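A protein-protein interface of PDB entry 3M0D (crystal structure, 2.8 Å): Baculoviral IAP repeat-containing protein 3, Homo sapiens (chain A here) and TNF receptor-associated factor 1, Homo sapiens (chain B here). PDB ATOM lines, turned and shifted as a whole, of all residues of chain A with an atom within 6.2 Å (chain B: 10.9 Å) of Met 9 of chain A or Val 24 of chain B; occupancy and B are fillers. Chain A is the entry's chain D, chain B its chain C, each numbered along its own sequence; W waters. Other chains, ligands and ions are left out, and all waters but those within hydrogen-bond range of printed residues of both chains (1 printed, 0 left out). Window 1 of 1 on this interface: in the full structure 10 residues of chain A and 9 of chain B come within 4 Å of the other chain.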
ATOM      1  N   CYS A   4       1.133  15.996  -0.306  1.00  0.00           N
ATOM      2  CA  CYS A   4       0.144  15.967  -1.364  1.00  0.00           C
ATOM      3  C   CYS A   4      -0.610  14.648  -1.392  1.00  0.00           C
ATOM      4  O   CYS A   4      -1.798  14.641  -1.701  1.00  0.00           O
ATOM      5  CB  CYS A   4       0.803  16.227  -2.714  1.00  0.00           C
ATOM      6  SG  CYS A   4       1.213  17.951  -2.958  1.00  0.00           S
ATOM      7  N   GLU A   5       0.072  13.538  -1.083  1.00  0.00           N
ATOM      8  CA  GLU A   5      -0.605  12.239  -0.916  1.00  0.00           C
ATOM      9  C   GLU A   5      -1.733  12.262   0.137  1.00  0.00           C
ATOM     10  O   GLU A   5      -2.849  11.801  -0.123  1.00  0.00           O
ATOM     11  CB  GLU A   5       0.404  11.168  -0.542  1.00  0.00           C
ATOM     12  CG  GLU A   5      -0.168   9.778  -0.413  1.00  0.00           C
ATOM     13  CD  GLU A   5       0.938   8.729  -0.354  1.00  0.00           C
ATOM     14  OE1 GLU A   5       0.653   7.555   0.011  1.00  0.00           O
ATOM     15  OE2 GLU A   5       2.098   9.092  -0.685  1.00  0.00           O
ATOM     16  N   LEU A   6      -1.439  12.799   1.320  1.00  0.00           N
ATOM     17  CA  LEU A   6      -2.455  12.946   2.362  1.00  0.00           C
ATOM     18  C   LEU A   6      -3.642  13.832   1.950  1.00  0.00           C
ATOM     19  O   LEU A   6      -4.798  13.481   2.159  1.00  0.00           O
ATOM     20  CB  LEU A   6      -1.823  13.456   3.655  1.00  0.00           C
ATOM     21  CG  LEU A   6      -1.234  12.296   4.458  1.00  0.00           C
ATOM     22  CD1 LEU A   6      -0.410  12.758   5.637  1.00  0.00           C
ATOM     23  CD2 LEU A   6      -2.349  11.417   4.936  1.00  0.00           C
ATOM     24  N   TYR A   7      -3.347  14.977   1.358  1.00  0.00           N
ATOM     25  CA  TYR A   7      -4.387  15.841   0.845  1.00  0.00           C
ATOM     26  C   TYR A   7      -5.243  15.131  -0.200  1.00  0.00           C
ATOM     27  O   TYR A   7      -6.457  15.355  -0.271  1.00  0.00           O
ATOM     28  CB  TYR A   7      -3.762  17.108   0.268  1.00  0.00           C
ATOM     29  CG  TYR A   7      -3.529  18.188   1.290  1.00  0.00           C
ATOM     30  CD1 TYR A   7      -2.541  18.054   2.258  1.00  0.00           C
ATOM     31  CD2 TYR A   7      -4.300  19.361   1.282  1.00  0.00           C
ATOM     32  CE1 TYR A   7      -2.325  19.063   3.201  1.00  0.00           C
ATOM     33  CE2 TYR A   7      -4.097  20.376   2.219  1.00  0.00           C
ATOM     34  CZ  TYR A   7      -3.107  20.221   3.174  1.00  0.00           C
ATOM     35  OH  TYR A   7      -2.908  21.213   4.104  1.00  0.00           O
ATOM     36  N   ARG A   8      -4.610  14.294  -1.017  1.00  0.00           N
ATOM     37  CA  ARG A   8      -5.341  13.430  -1.947  1.00  0.00           C
ATOM     38  C   ARG A   8      -6.182  12.396  -1.201  1.00  0.00           C
ATOM     39  O   ARG A   8      -7.311  12.114  -1.591  1.00  0.00           O
ATOM     40  CB  ARG A   8      -4.391  12.719  -2.920  1.00  0.00           C
ATOM     41  CG  ARG A   8      -4.154  13.473  -4.223  1.00  0.00           C
ATOM     42  CD  ARG A   8      -3.547  12.549  -5.275  1.00  0.00           C
ATOM     43  NE  ARG A   8      -2.339  11.857  -4.803  1.00  0.00           N
ATOM     44  CZ  ARG A   8      -1.120  12.412  -4.718  1.00  0.00           C
ATOM     45  NH1 ARG A   8      -0.917  13.695  -5.055  1.00  0.00           N
ATOM     46  NH2 ARG A   8      -0.098  11.688  -4.269  1.00  0.00           N
ATOM     47  N   MET A   9      -5.633  11.830  -0.129  1.00  0.00           N
ATOM     48  CA  MET A   9      -6.364  10.846   0.648  1.00  0.00           C
ATOM     49  C   MET A   9      -7.620  11.451   1.255  1.00  0.00           C
ATOM     50  O   MET A   9      -8.683  10.849   1.212  1.00  0.00           O
ATOM     51  CB  MET A   9      -5.492  10.320   1.763  1.00  0.00           C
ATOM     52  CG  MET A   9      -5.807   8.902   2.169  1.00  0.00           C
ATOM     53  SD  MET A   9      -5.006   8.520   3.747  1.00  0.00           S
ATOM     54  CE  MET A   9      -5.284   6.760   3.777  1.00  0.00           C
ATOM     55  N   SER A  10      -7.488  12.641   1.832  1.00  0.00           N
ATOM     56  CA  SER A  10      -8.603  13.316   2.493  1.00  0.00           C
ATOM     57  C   SER A  10      -9.844  13.442   1.594  1.00  0.00           C
ATOM     58  O   SER A  10     -10.941  13.766   2.083  1.00  0.00           O
ATOM     59  CB  SER A  10      -8.178  14.692   3.016  1.00  0.00           C
ATOM     60  OG  SER A  10      -8.145  15.655   1.974  1.00  0.00           O
ATOM     61  N   THR A  11      -9.680  13.172   0.296  1.00  0.00           N
ATOM     62  CA  THR A  11     -10.815  13.255  -0.634  1.00  0.00           C
ATOM     63  C   THR A  11     -11.663  11.982  -0.642  1.00  0.00           C
ATOM     64  O   THR A  11     -12.589  11.825  -1.455  1.00  0.00           O
ATOM     65  CB  THR A  11     -10.392  13.616  -2.086  1.00  0.00           C
ATOM     66  OG1 THR A  11      -9.634  12.548  -2.677  1.00  0.00           O
ATOM     67  CG2 THR A  11      -9.578  14.921  -2.107  1.00  0.00           C
ATOM     68  N   TYR A  12     -11.346  11.073   0.273  1.00  0.00           N
ATOM     69  CA  TYR A  12     -11.936   9.741   0.239  1.00  0.00           C
ATOM     70  C   TYR A  12     -12.895   9.447   1.422  1.00  0.00           C
ATOM     71  O   TYR A  12     -13.243   8.295   1.687  1.00  0.00           O
ATOM     72  CB  TYR A  12     -10.818   8.680   0.137  1.00  0.00           C
ATOM     73  CG  TYR A  12     -10.139   8.580  -1.220  1.00  0.00           C
ATOM     74  CD1 TYR A  12     -10.617   7.705  -2.198  1.00  0.00           C
ATOM     75  CD2 TYR A  12      -8.997   9.335  -1.513  1.00  0.00           C
ATOM     76  CE1 TYR A  12      -9.990   7.595  -3.442  1.00  0.00           C
ATOM     77  CE2 TYR A  12      -8.369   9.244  -2.747  1.00  0.00           C
ATOM     78  CZ  TYR A  12      -8.868   8.375  -3.711  1.00  0.00           C
ATOM     79  OH  TYR A  12      -8.245   8.276  -4.937  1.00  0.00           O
ATOM     80  N   SER A  13     -13.325  10.490   2.117  1.00  0.00           N
ATOM     81  CA  SER A  13     -14.158  10.314   3.301  1.00  0.00           C
ATOM     82  C   SER A  13     -15.496   9.706   2.921  1.00  0.00           C
ATOM     83  O   SER A  13     -16.154   9.065   3.747  1.00  0.00           O
ATOM     84  CB  SER A  13     -14.375  11.650   4.026  1.00  0.00           C
ATOM     85  OG  SER A  13     -14.891  12.627   3.142  1.00  0.00           O
ATOM     86  N   THR A  14     -15.876   9.907   1.660  1.00  0.00           N
ATOM     87  CA  THR A  14     -17.208   9.566   1.156  1.00  0.00           C
ATOM     88  C   THR A  14     -17.153   8.437   0.137  1.00  0.00           C
ATOM     89  O   THR A  14     -18.058   8.281  -0.685  1.00  0.00           O
ATOM     90  CB  THR A  14     -17.850  10.798   0.511  1.00  0.00           C
ATOM     91  OG1 THR A  14     -16.881  11.457  -0.326  1.00  0.00           O
ATOM     92  CG2 THR A  14     -18.304  11.764   1.596  1.00  0.00           C
ATOM     93  N   GLU A  23      -8.324   3.125  -0.046  1.00  0.00           N
ATOM     94  CA  GLU A  23      -8.202   4.514  -0.458  1.00  0.00           C
ATOM     95  C   GLU A  23      -6.765   4.940  -0.329  1.00  0.00           C
ATOM     96  O   GLU A  23      -6.363   5.927  -0.934  1.00  0.00           O
ATOM     97  CB  GLU A  23      -9.097   5.421   0.369  1.00  0.00           C
ATOM     98  CG  GLU A  23     -10.561   5.038   0.308  1.00  0.00           C
ATOM     99  CD  GLU A  23     -10.962   4.122   1.444  1.00  0.00           C
ATOM    100  OE1 GLU A  23     -10.065   3.491   2.049  1.00  0.00           O
ATOM    101  OE2 GLU A  23     -12.175   4.048   1.741  1.00  0.00           O
ATOM    102  N   ARG A  24      -5.989   4.168   0.433  1.00  0.00           N
ATOM    103  CA  ARG A  24      -4.583   4.498   0.648  1.00  0.00           C
ATOM    104  C   ARG A  24      -3.729   4.334  -0.595  1.00  0.00           C
ATOM    105  O   ARG A  24      -3.022   5.251  -0.985  1.00  0.00           O
ATOM    106  CB  ARG A  24      -3.970   3.728   1.811  1.00  0.00           C
ATOM    107  CG  ARG A  24      -2.505   4.126   2.038  1.00  0.00           C
ATOM    108  CD  ARG A  24      -1.840   3.423   3.214  1.00  0.00           C
ATOM    109  NE  ARG A  24      -2.449   3.786   4.483  1.00  0.00           N
ATOM    110  CZ  ARG A  24      -2.105   4.852   5.195  1.00  0.00           C
ATOM    111  NH1 ARG A  24      -1.135   5.645   4.763  1.00  0.00           N
ATOM    112  NH2 ARG A  24      -2.720   5.114   6.344  1.00  0.00           N
ATOM    113  N   ALA A  27      -4.743   6.816  -3.394  1.00  0.00           N
ATOM    114  CA  ALA A  27      -4.103   8.103  -3.218  1.00  0.00           C
ATOM    115  C   ALA A  27      -2.569   8.061  -3.527  1.00  0.00           C
ATOM    116  O   ALA A  27      -2.038   8.924  -4.228  1.00  0.00           O
ATOM    117  CB  ALA A  27      -4.392   8.618  -1.814  1.00  0.00           C
ATOM    118  N   PHE A  31      -4.245   9.359  -7.463  1.00  0.00           N
ATOM    119  CA  PHE A  31      -5.648   9.634  -7.767  1.00  0.00           C
ATOM    120  C   PHE A  31      -6.389  10.266  -6.591  1.00  0.00           C
ATOM    121  O   PHE A  31      -6.171   9.881  -5.430  1.00  0.00           O
ATOM    122  CB  PHE A  31      -6.370   8.342  -8.149  1.00  0.00           C
ATOM    123  CG  PHE A  31      -5.770   7.623  -9.320  1.00  0.00           C
ATOM    124  CD1 PHE A  31      -5.915   8.129 -10.612  1.00  0.00           C
ATOM    125  CD2 PHE A  31      -5.083   6.420  -9.139  1.00  0.00           C
ATOM    126  CE1 PHE A  31      -5.367   7.456 -11.710  1.00  0.00           C
ATOM    127  CE2 PHE A  31      -4.535   5.752 -10.224  1.00  0.00           C
ATOM    128  CZ  PHE A  31      -4.683   6.269 -11.511  1.00  0.00           C
ATOM    129  N   ARG B  16     -10.713  21.020   8.020  1.00  0.00           N
ATOM    130  CA  ARG B  16     -11.573  20.169   7.204  1.00  0.00           C
ATOM    131  C   ARG B  16     -10.750  19.032   6.617  1.00  0.00           C
ATOM    132  O   ARG B  16     -11.227  17.892   6.540  1.00  0.00           O
ATOM    133  CB  ARG B  16     -12.293  20.933   6.096  1.00  0.00           C
ATOM    134  N   VAL B  17      -9.514  19.331   6.211  1.00  0.00           N
ATOM    135  CA  VAL B  17      -8.676  18.314   5.581  1.00  0.00           C
ATOM    136  C   VAL B  17      -8.316  17.275   6.612  1.00  0.00           C
ATOM    137  O   VAL B  17      -8.391  16.075   6.352  1.00  0.00           O
ATOM    138  CB  VAL B  17      -7.360  18.900   5.024  1.00  0.00           C
ATOM    139  CG1 VAL B  17      -6.318  17.782   4.755  1.00  0.00           C
ATOM    140  CG2 VAL B  17      -7.621  19.724   3.782  1.00  0.00           C
ATOM    141  N   PHE B  18      -7.913  17.745   7.784  1.00  0.00           N
ATOM    142  CA  PHE B  18      -7.582  16.849   8.868  1.00  0.00           C
ATOM    143  C   PHE B  18      -8.749  15.945   9.233  1.00  0.00           C
ATOM    144  O   PHE B  18      -8.567  14.746   9.458  1.00  0.00           O
ATOM    145  CB  PHE B  18      -7.165  17.632  10.097  1.00  0.00           C
ATOM    146  CG  PHE B  18      -5.931  18.440   9.917  1.00  0.00           C
ATOM    147  CD1 PHE B  18      -5.020  18.132   8.916  1.00  0.00           C
ATOM    148  CD2 PHE B  18      -5.675  19.520  10.759  1.00  0.00           C
ATOM    149  CE1 PHE B  18      -3.863  18.878   8.762  1.00  0.00           C
ATOM    150  CE2 PHE B  18      -4.524  20.264  10.613  1.00  0.00           C
ATOM    151  CZ  PHE B  18      -3.615  19.943   9.620  1.00  0.00           C
ATOM    152  N   GLU B  19      -9.950  16.508   9.304  1.00  0.00           N
ATOM    153  CA  GLU B  19     -11.073  15.687   9.723  1.00  0.00           C
ATOM    154  C   GLU B  19     -11.421  14.647   8.639  1.00  0.00           C
ATOM    155  O   GLU B  19     -11.777  13.510   8.957  1.00  0.00           O
ATOM    156  CB  GLU B  19     -12.259  16.533  10.247  1.00  0.00           C
ATOM    157  CG  GLU B  19     -13.608  16.327   9.566  1.00  0.00           C
ATOM    158  CD  GLU B  19     -14.231  17.649   9.092  1.00  0.00           C
ATOM    159  OE1 GLU B  19     -14.101  18.660   9.823  1.00  0.00           O
ATOM    160  OE2 GLU B  19     -14.829  17.681   7.985  1.00  0.00           O
ATOM    161  N   ASN B  20     -11.263  15.005   7.367  1.00  0.00           N
ATOM    162  CA  ASN B  20     -11.507  14.037   6.303  1.00  0.00           C
ATOM    163  C   ASN B  20     -10.457  12.920   6.280  1.00  0.00           C
ATOM    164  O   ASN B  20     -10.776  11.754   6.041  1.00  0.00           O
ATOM    165  CB  ASN B  20     -11.557  14.708   4.936  1.00  0.00           C
ATOM    166  CG  ASN B  20     -12.697  15.699   4.815  1.00  0.00           C
ATOM    167  OD1 ASN B  20     -12.621  16.683   4.053  1.00  0.00           O
ATOM    168  ND2 ASN B  20     -13.773  15.446   5.570  1.00  0.00           N
ATOM    169  N   ILE B  21      -9.197  13.276   6.509  1.00  0.00           N
ATOM    170  CA  ILE B  21      -8.152  12.272   6.471  1.00  0.00           C
ATOM    171  C   ILE B  21      -8.437  11.295   7.580  1.00  0.00           C
ATOM    172  O   ILE B  21      -8.445  10.099   7.371  1.00  0.00           O
ATOM    173  CB  ILE B  21      -6.737  12.871   6.631  1.00  0.00           C
ATOM    174  CG1 ILE B  21      -6.342  13.636   5.368  1.00  0.00           C
ATOM    175  CG2 ILE B  21      -5.713  11.762   6.894  1.00  0.00           C
ATOM    176  CD1 ILE B  21      -5.016  14.362   5.477  1.00  0.00           C
ATOM    177  N   VAL B  22      -8.691  11.820   8.765  1.00  0.00           N
ATOM    178  CA  VAL B  22      -9.043  10.982   9.904  1.00  0.00           C
ATOM    179  C   VAL B  22     -10.264  10.051   9.648  1.00  0.00           C
ATOM    180  O   VAL B  22     -10.295   8.911  10.111  1.00  0.00           O
ATOM    181  CB  VAL B  22      -9.239  11.842  11.166  1.00  0.00           C
ATOM    182  CG1 VAL B  22      -9.984  11.070  12.209  1.00  0.00           C
ATOM    183  CG2 VAL B  22      -7.911  12.281  11.716  1.00  0.00           C
ATOM    184  N   ALA B  23     -11.257  10.541   8.911  1.00  0.00           N
ATOM    185  CA  ALA B  23     -12.380   9.711   8.470  1.00  0.00           C
ATOM    186  C   ALA B  23     -11.884   8.447   7.742  1.00  0.00           C
ATOM    187  O   ALA B  23     -12.273   7.311   8.044  1.00  0.00           O
ATOM    188  CB  ALA B  23     -13.291  10.518   7.544  1.00  0.00           C
ATOM    189  N   VAL B  24     -11.026   8.682   6.760  1.00  0.00           N
ATOM    190  CA  VAL B  24     -10.427   7.634   5.968  1.00  0.00           C
ATOM    191  C   VAL B  24      -9.623   6.693   6.861  1.00  0.00           C
ATOM    192  O   VAL B  24      -9.805   5.485   6.810  1.00  0.00           O
ATOM    193  CB  VAL B  24      -9.538   8.270   4.903  1.00  0.00           C
ATOM    194  CG1 VAL B  24      -9.031   7.250   3.948  1.00  0.00           C
ATOM    195  CG2 VAL B  24     -10.334   9.324   4.154  1.00  0.00           C
ATOM    196  N   LEU B  25      -8.743   7.254   7.684  1.00  0.00           N
ATOM    197  CA  LEU B  25      -7.958   6.458   8.623  1.00  0.00           C
ATOM    198  C   LEU B  25      -8.868   5.604   9.492  1.00  0.00           C
ATOM    199  O   LEU B  25      -8.602   4.414   9.723  1.00  0.00           O
ATOM    200  CB  LEU B  25      -7.066   7.343   9.502  1.00  0.00           C
ATOM    201  CG  LEU B  25      -5.851   7.963   8.805  1.00  0.00           C
ATOM    202  CD1 LEU B  25      -4.848   8.474   9.809  1.00  0.00           C
ATOM    203  CD2 LEU B  25      -5.178   6.973   7.910  1.00  0.00           C
ATOM    204  N   ASN B  26      -9.943   6.222   9.977  1.00  0.00           N
ATOM    205  CA  ASN B  26     -10.961   5.501  10.721  1.00  0.00           C
ATOM    206  C   ASN B  26     -11.460   4.284   9.941  1.00  0.00           C
ATOM    207  O   ASN B  26     -11.520   3.175  10.474  1.00  0.00           O
ATOM    208  CB  ASN B  26     -12.109   6.426  11.062  1.00  0.00           C
ATOM    209  CG  ASN B  26     -13.277   5.691  11.654  1.00  0.00           C
ATOM    210  OD1 ASN B  26     -13.150   5.031  12.693  1.00  0.00           O
ATOM    211  ND2 ASN B  26     -14.438   5.804  11.009  1.00  0.00           N
ATOM    212  N   LYS B  27     -11.789   4.486   8.668  1.00  0.00           N
ATOM    213  CA  LYS B  27     -12.216   3.383   7.804  1.00  0.00           C
ATOM    214  C   LYS B  27     -11.156   2.299   7.650  1.00  0.00           C
ATOM    215  O   LYS B  27     -11.465   1.114   7.622  1.00  0.00           O
ATOM    216  CB  LYS B  27     -12.594   3.889   6.415  1.00  0.00           C
ATOM    217  CG  LYS B  27     -13.943   4.567   6.346  1.00  0.00           C
ATOM    218  CD  LYS B  27     -14.193   5.084   4.945  1.00  0.00           C
ATOM    219  CE  LYS B  27     -15.670   5.330   4.702  1.00  0.00           C
ATOM    220  NZ  LYS B  27     -15.865   6.049   3.416  1.00  0.00           N
ATOM    221  N   GLU B  28      -9.903   2.721   7.531  1.00  0.00           N
ATOM    222  CA  GLU B  28      -8.811   1.789   7.337  1.00  0.00           C
ATOM    223  C   GLU B  28      -8.695   0.859   8.536  1.00  0.00           C
ATOM    224  O   GLU B  28      -8.655  -0.365   8.390  1.00  0.00           O
ATOM    225  CB  GLU B  28      -7.511   2.550   7.141  1.00  0.00           C
ATOM    226  CG  GLU B  28      -6.391   1.706   6.577  1.00  0.00           C
ATOM    227  CD  GLU B  28      -5.233   2.549   6.129  1.00  0.00           C
ATOM    228  OE1 GLU B  28      -5.404   3.792   6.072  1.00  0.00           O
ATOM    229  OE2 GLU B  28      -4.156   1.974   5.839  1.00  0.00           O
ATOM    230  N   VAL B  29      -8.645   1.461   9.718  1.00  0.00           N
ATOM    231  CA  VAL B  29      -8.573   0.727  10.973  1.00  0.00           C
ATOM    232  C   VAL B  29      -9.701  -0.325  11.083  1.00  0.00           C
ATOM    233  O   VAL B  29      -9.503  -1.420  11.627  1.00  0.00           O
ATOM    234  CB  VAL B  29      -8.595   1.718  12.188  1.00  0.00           C
ATOM    235  CG1 VAL B  29      -8.936   1.016  13.480  1.00  0.00           C
ATOM    236  CG2 VAL B  29      -7.269   2.414  12.338  1.00  0.00           C
ATOM    237  N   GLU B  30     -10.873   0.006  10.547  1.00  0.00           N
ATOM    238  CA  GLU B  30     -12.042  -0.846  10.673  1.00  0.00           C
ATOM    239  C   GLU B  30     -11.941  -2.113   9.810  1.00  0.00           C
ATOM    240  O   GLU B  30     -12.181  -3.227  10.277  1.00  0.00           O
ATOM    241  CB  GLU B  30     -13.300  -0.044  10.319  1.00  0.00           C
ATOM    242  CG  GLU B  30     -14.591  -0.735  10.734  1.00  0.00           C
ATOM    243  CD  GLU B  30     -14.444  -1.468  12.058  1.00  0.00           C
ATOM    244  OE1 GLU B  30     -13.887  -0.859  13.006  1.00  0.00           O
ATOM    245  OE2 GLU B  30     -14.874  -2.648  12.144  1.00  0.00           O
ATOM    246  N   ALA B  31     -11.600  -1.919   8.540  1.00  0.00           N
ATOM    247  CA  ALA B  31     -11.306  -3.013   7.625  1.00  0.00           C
ATOM    248  C   ALA B  31     -10.251  -3.975   8.212  1.00  0.00           C
ATOM    249  O   ALA B  31     -10.326  -5.191   8.004  1.00  0.00           O
ATOM    250  CB  ALA B  31     -10.841  -2.452   6.276  1.00  0.00           C
ATOM    251  N   SER B  32      -9.265  -3.416   8.919  1.00  0.00           N
ATOM    252  CA  SER B  32      -8.223  -4.199   9.579  1.00  0.00           C
ATOM    253  C   SER B  32      -8.838  -5.073  10.648  1.00  0.00           C
ATOM    254  O   SER B  32      -8.530  -6.254  10.748  1.00  0.00           O
ATOM    255  CB  SER B  32      -7.161  -3.293  10.227  1.00  0.00           C
ATOM    256  OG  SER B  32      -6.273  -2.747   9.273  1.00  0.00           O
HETATM  257  O   HOH W   1      -7.143   3.566   3.257  1.00  0.00           O
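Hydrophobic or aromatic side chains of chain A that line the printed part of chain B: Leu 6, Tyr 7 and Met 9. Of the 17 printed residues of chain B, 8 touch a printed residue of chain A. Printed residues of chain B that touch a printed residue of chain A: Val 17, Asn 20, Ile 21, Ala 23, Val 24, Leu 25, Lys 27 and Glu 28. Hydrophobic or aromatic side chains of chain B that line the printed part of chain A: Val 17, Ile 21, Ala 23, Val 24 and Leu 25.
O of Phe 31 of chain A is in hydrogen-bond range of OH of Tyr 12 of chain A (2.7 Å). O of Tyr 7 of chain A lies within hydrogen-bond range of OG of Ser 10 of chain A (2.8 Å). The side-chain hydroxyl (OG) of Ser 32 of chain B sits at hydrogen-bond distance from the backbone carbonyl oxygen (O) of Glu 28 of chain B, at 3.5 Å. ND2 of Asn 20 of chain B sits at hydrogen-bond distance from OE2 of Glu 19 of chain B, at 3.5 Å. O of Arg 16 of chain B sits close to OD1 of Asn 20 of chain B, 3.1 Å away.
Water W1 lies within hydrogen-bond range of the backbone NH (N) of Arg 24 of chain A, the side-chain carboxylate (OE1) of Glu 23 of chain A and the side-chain carboxylate (OE1) of Glu 28 of chain B.
OE2 of Glu 28 of chain B lies within salt-bridge range of NE of Arg 24 of chain A, 2.8 Å away. The backbone carbonyl oxygen of Ser 13 of chain A lies within hydrogen-bond range of the side-chain amino group of Lys 27 of chain B (3.0 Å).
Of the printed residues of chain B, Tyr 7 of chain A touches Val 17. Of chain B, only Val 24 (3.7 Å) and Glu 28 (3.8 Å) come within 4 Å of Met 9 of chain A. No residue of chain B comes within 4 Å of Thr 11 of chain A. Of the printed residues of chain B, Tyr 12 of chain A touches Val 24 and Lys 27. Arg 24 of chain A touches just these residues of chain B: Leu 25 and Glu 28. Of the printed residues of chain A, Asn 20 of chain B touches Ser 10 and Ser 13. Printed residues of chain A within 4 Å of Val 24 of chain B: Met 9, Tyr 12 and Ser 13. The nearest printed residue of chain A that does not touch Val 24 of chain B is Glu 23 of chain A (4.02 Å).
Among the printed residues, pairs that only touch across the chains: Ser 10 of chain A with Asn 20 of chain B (3.1 Å), Ser 10 of chain A with Ile 21 of chain B (3.2 Å), Leu 6 of chain A with Ile 21 of chain B (3.4 Å), Arg 24 of chain A with Leu 25 of chain B (3.5 Å), Ser 10 of chain A with Val 17 of chain B (3.6 Å), Met 9 of chain A with Val 24 of chain B (3.7 Å), Tyr 12 of chain A with Val 24 of chain B (3.7 Å), Met 9 of chain A with Glu 28 of chain B (3.8 Å), Ser 13 of chain A with Val 24 of chain B (3.8 Å), Ser 13 of chain A with Ala 23 of chain B (3.9 Å), Tyr 12 of chain A with Lys 27 of chain B (3.9 Å), Ser 13 of chain A with Asn 20 of chain B (3.9 Å), Tyr 7 of chain A with Val 17 of chain B (3.9 Å) and Glu 23 of chain A with Lys 27 of chain B (3.9 Å).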
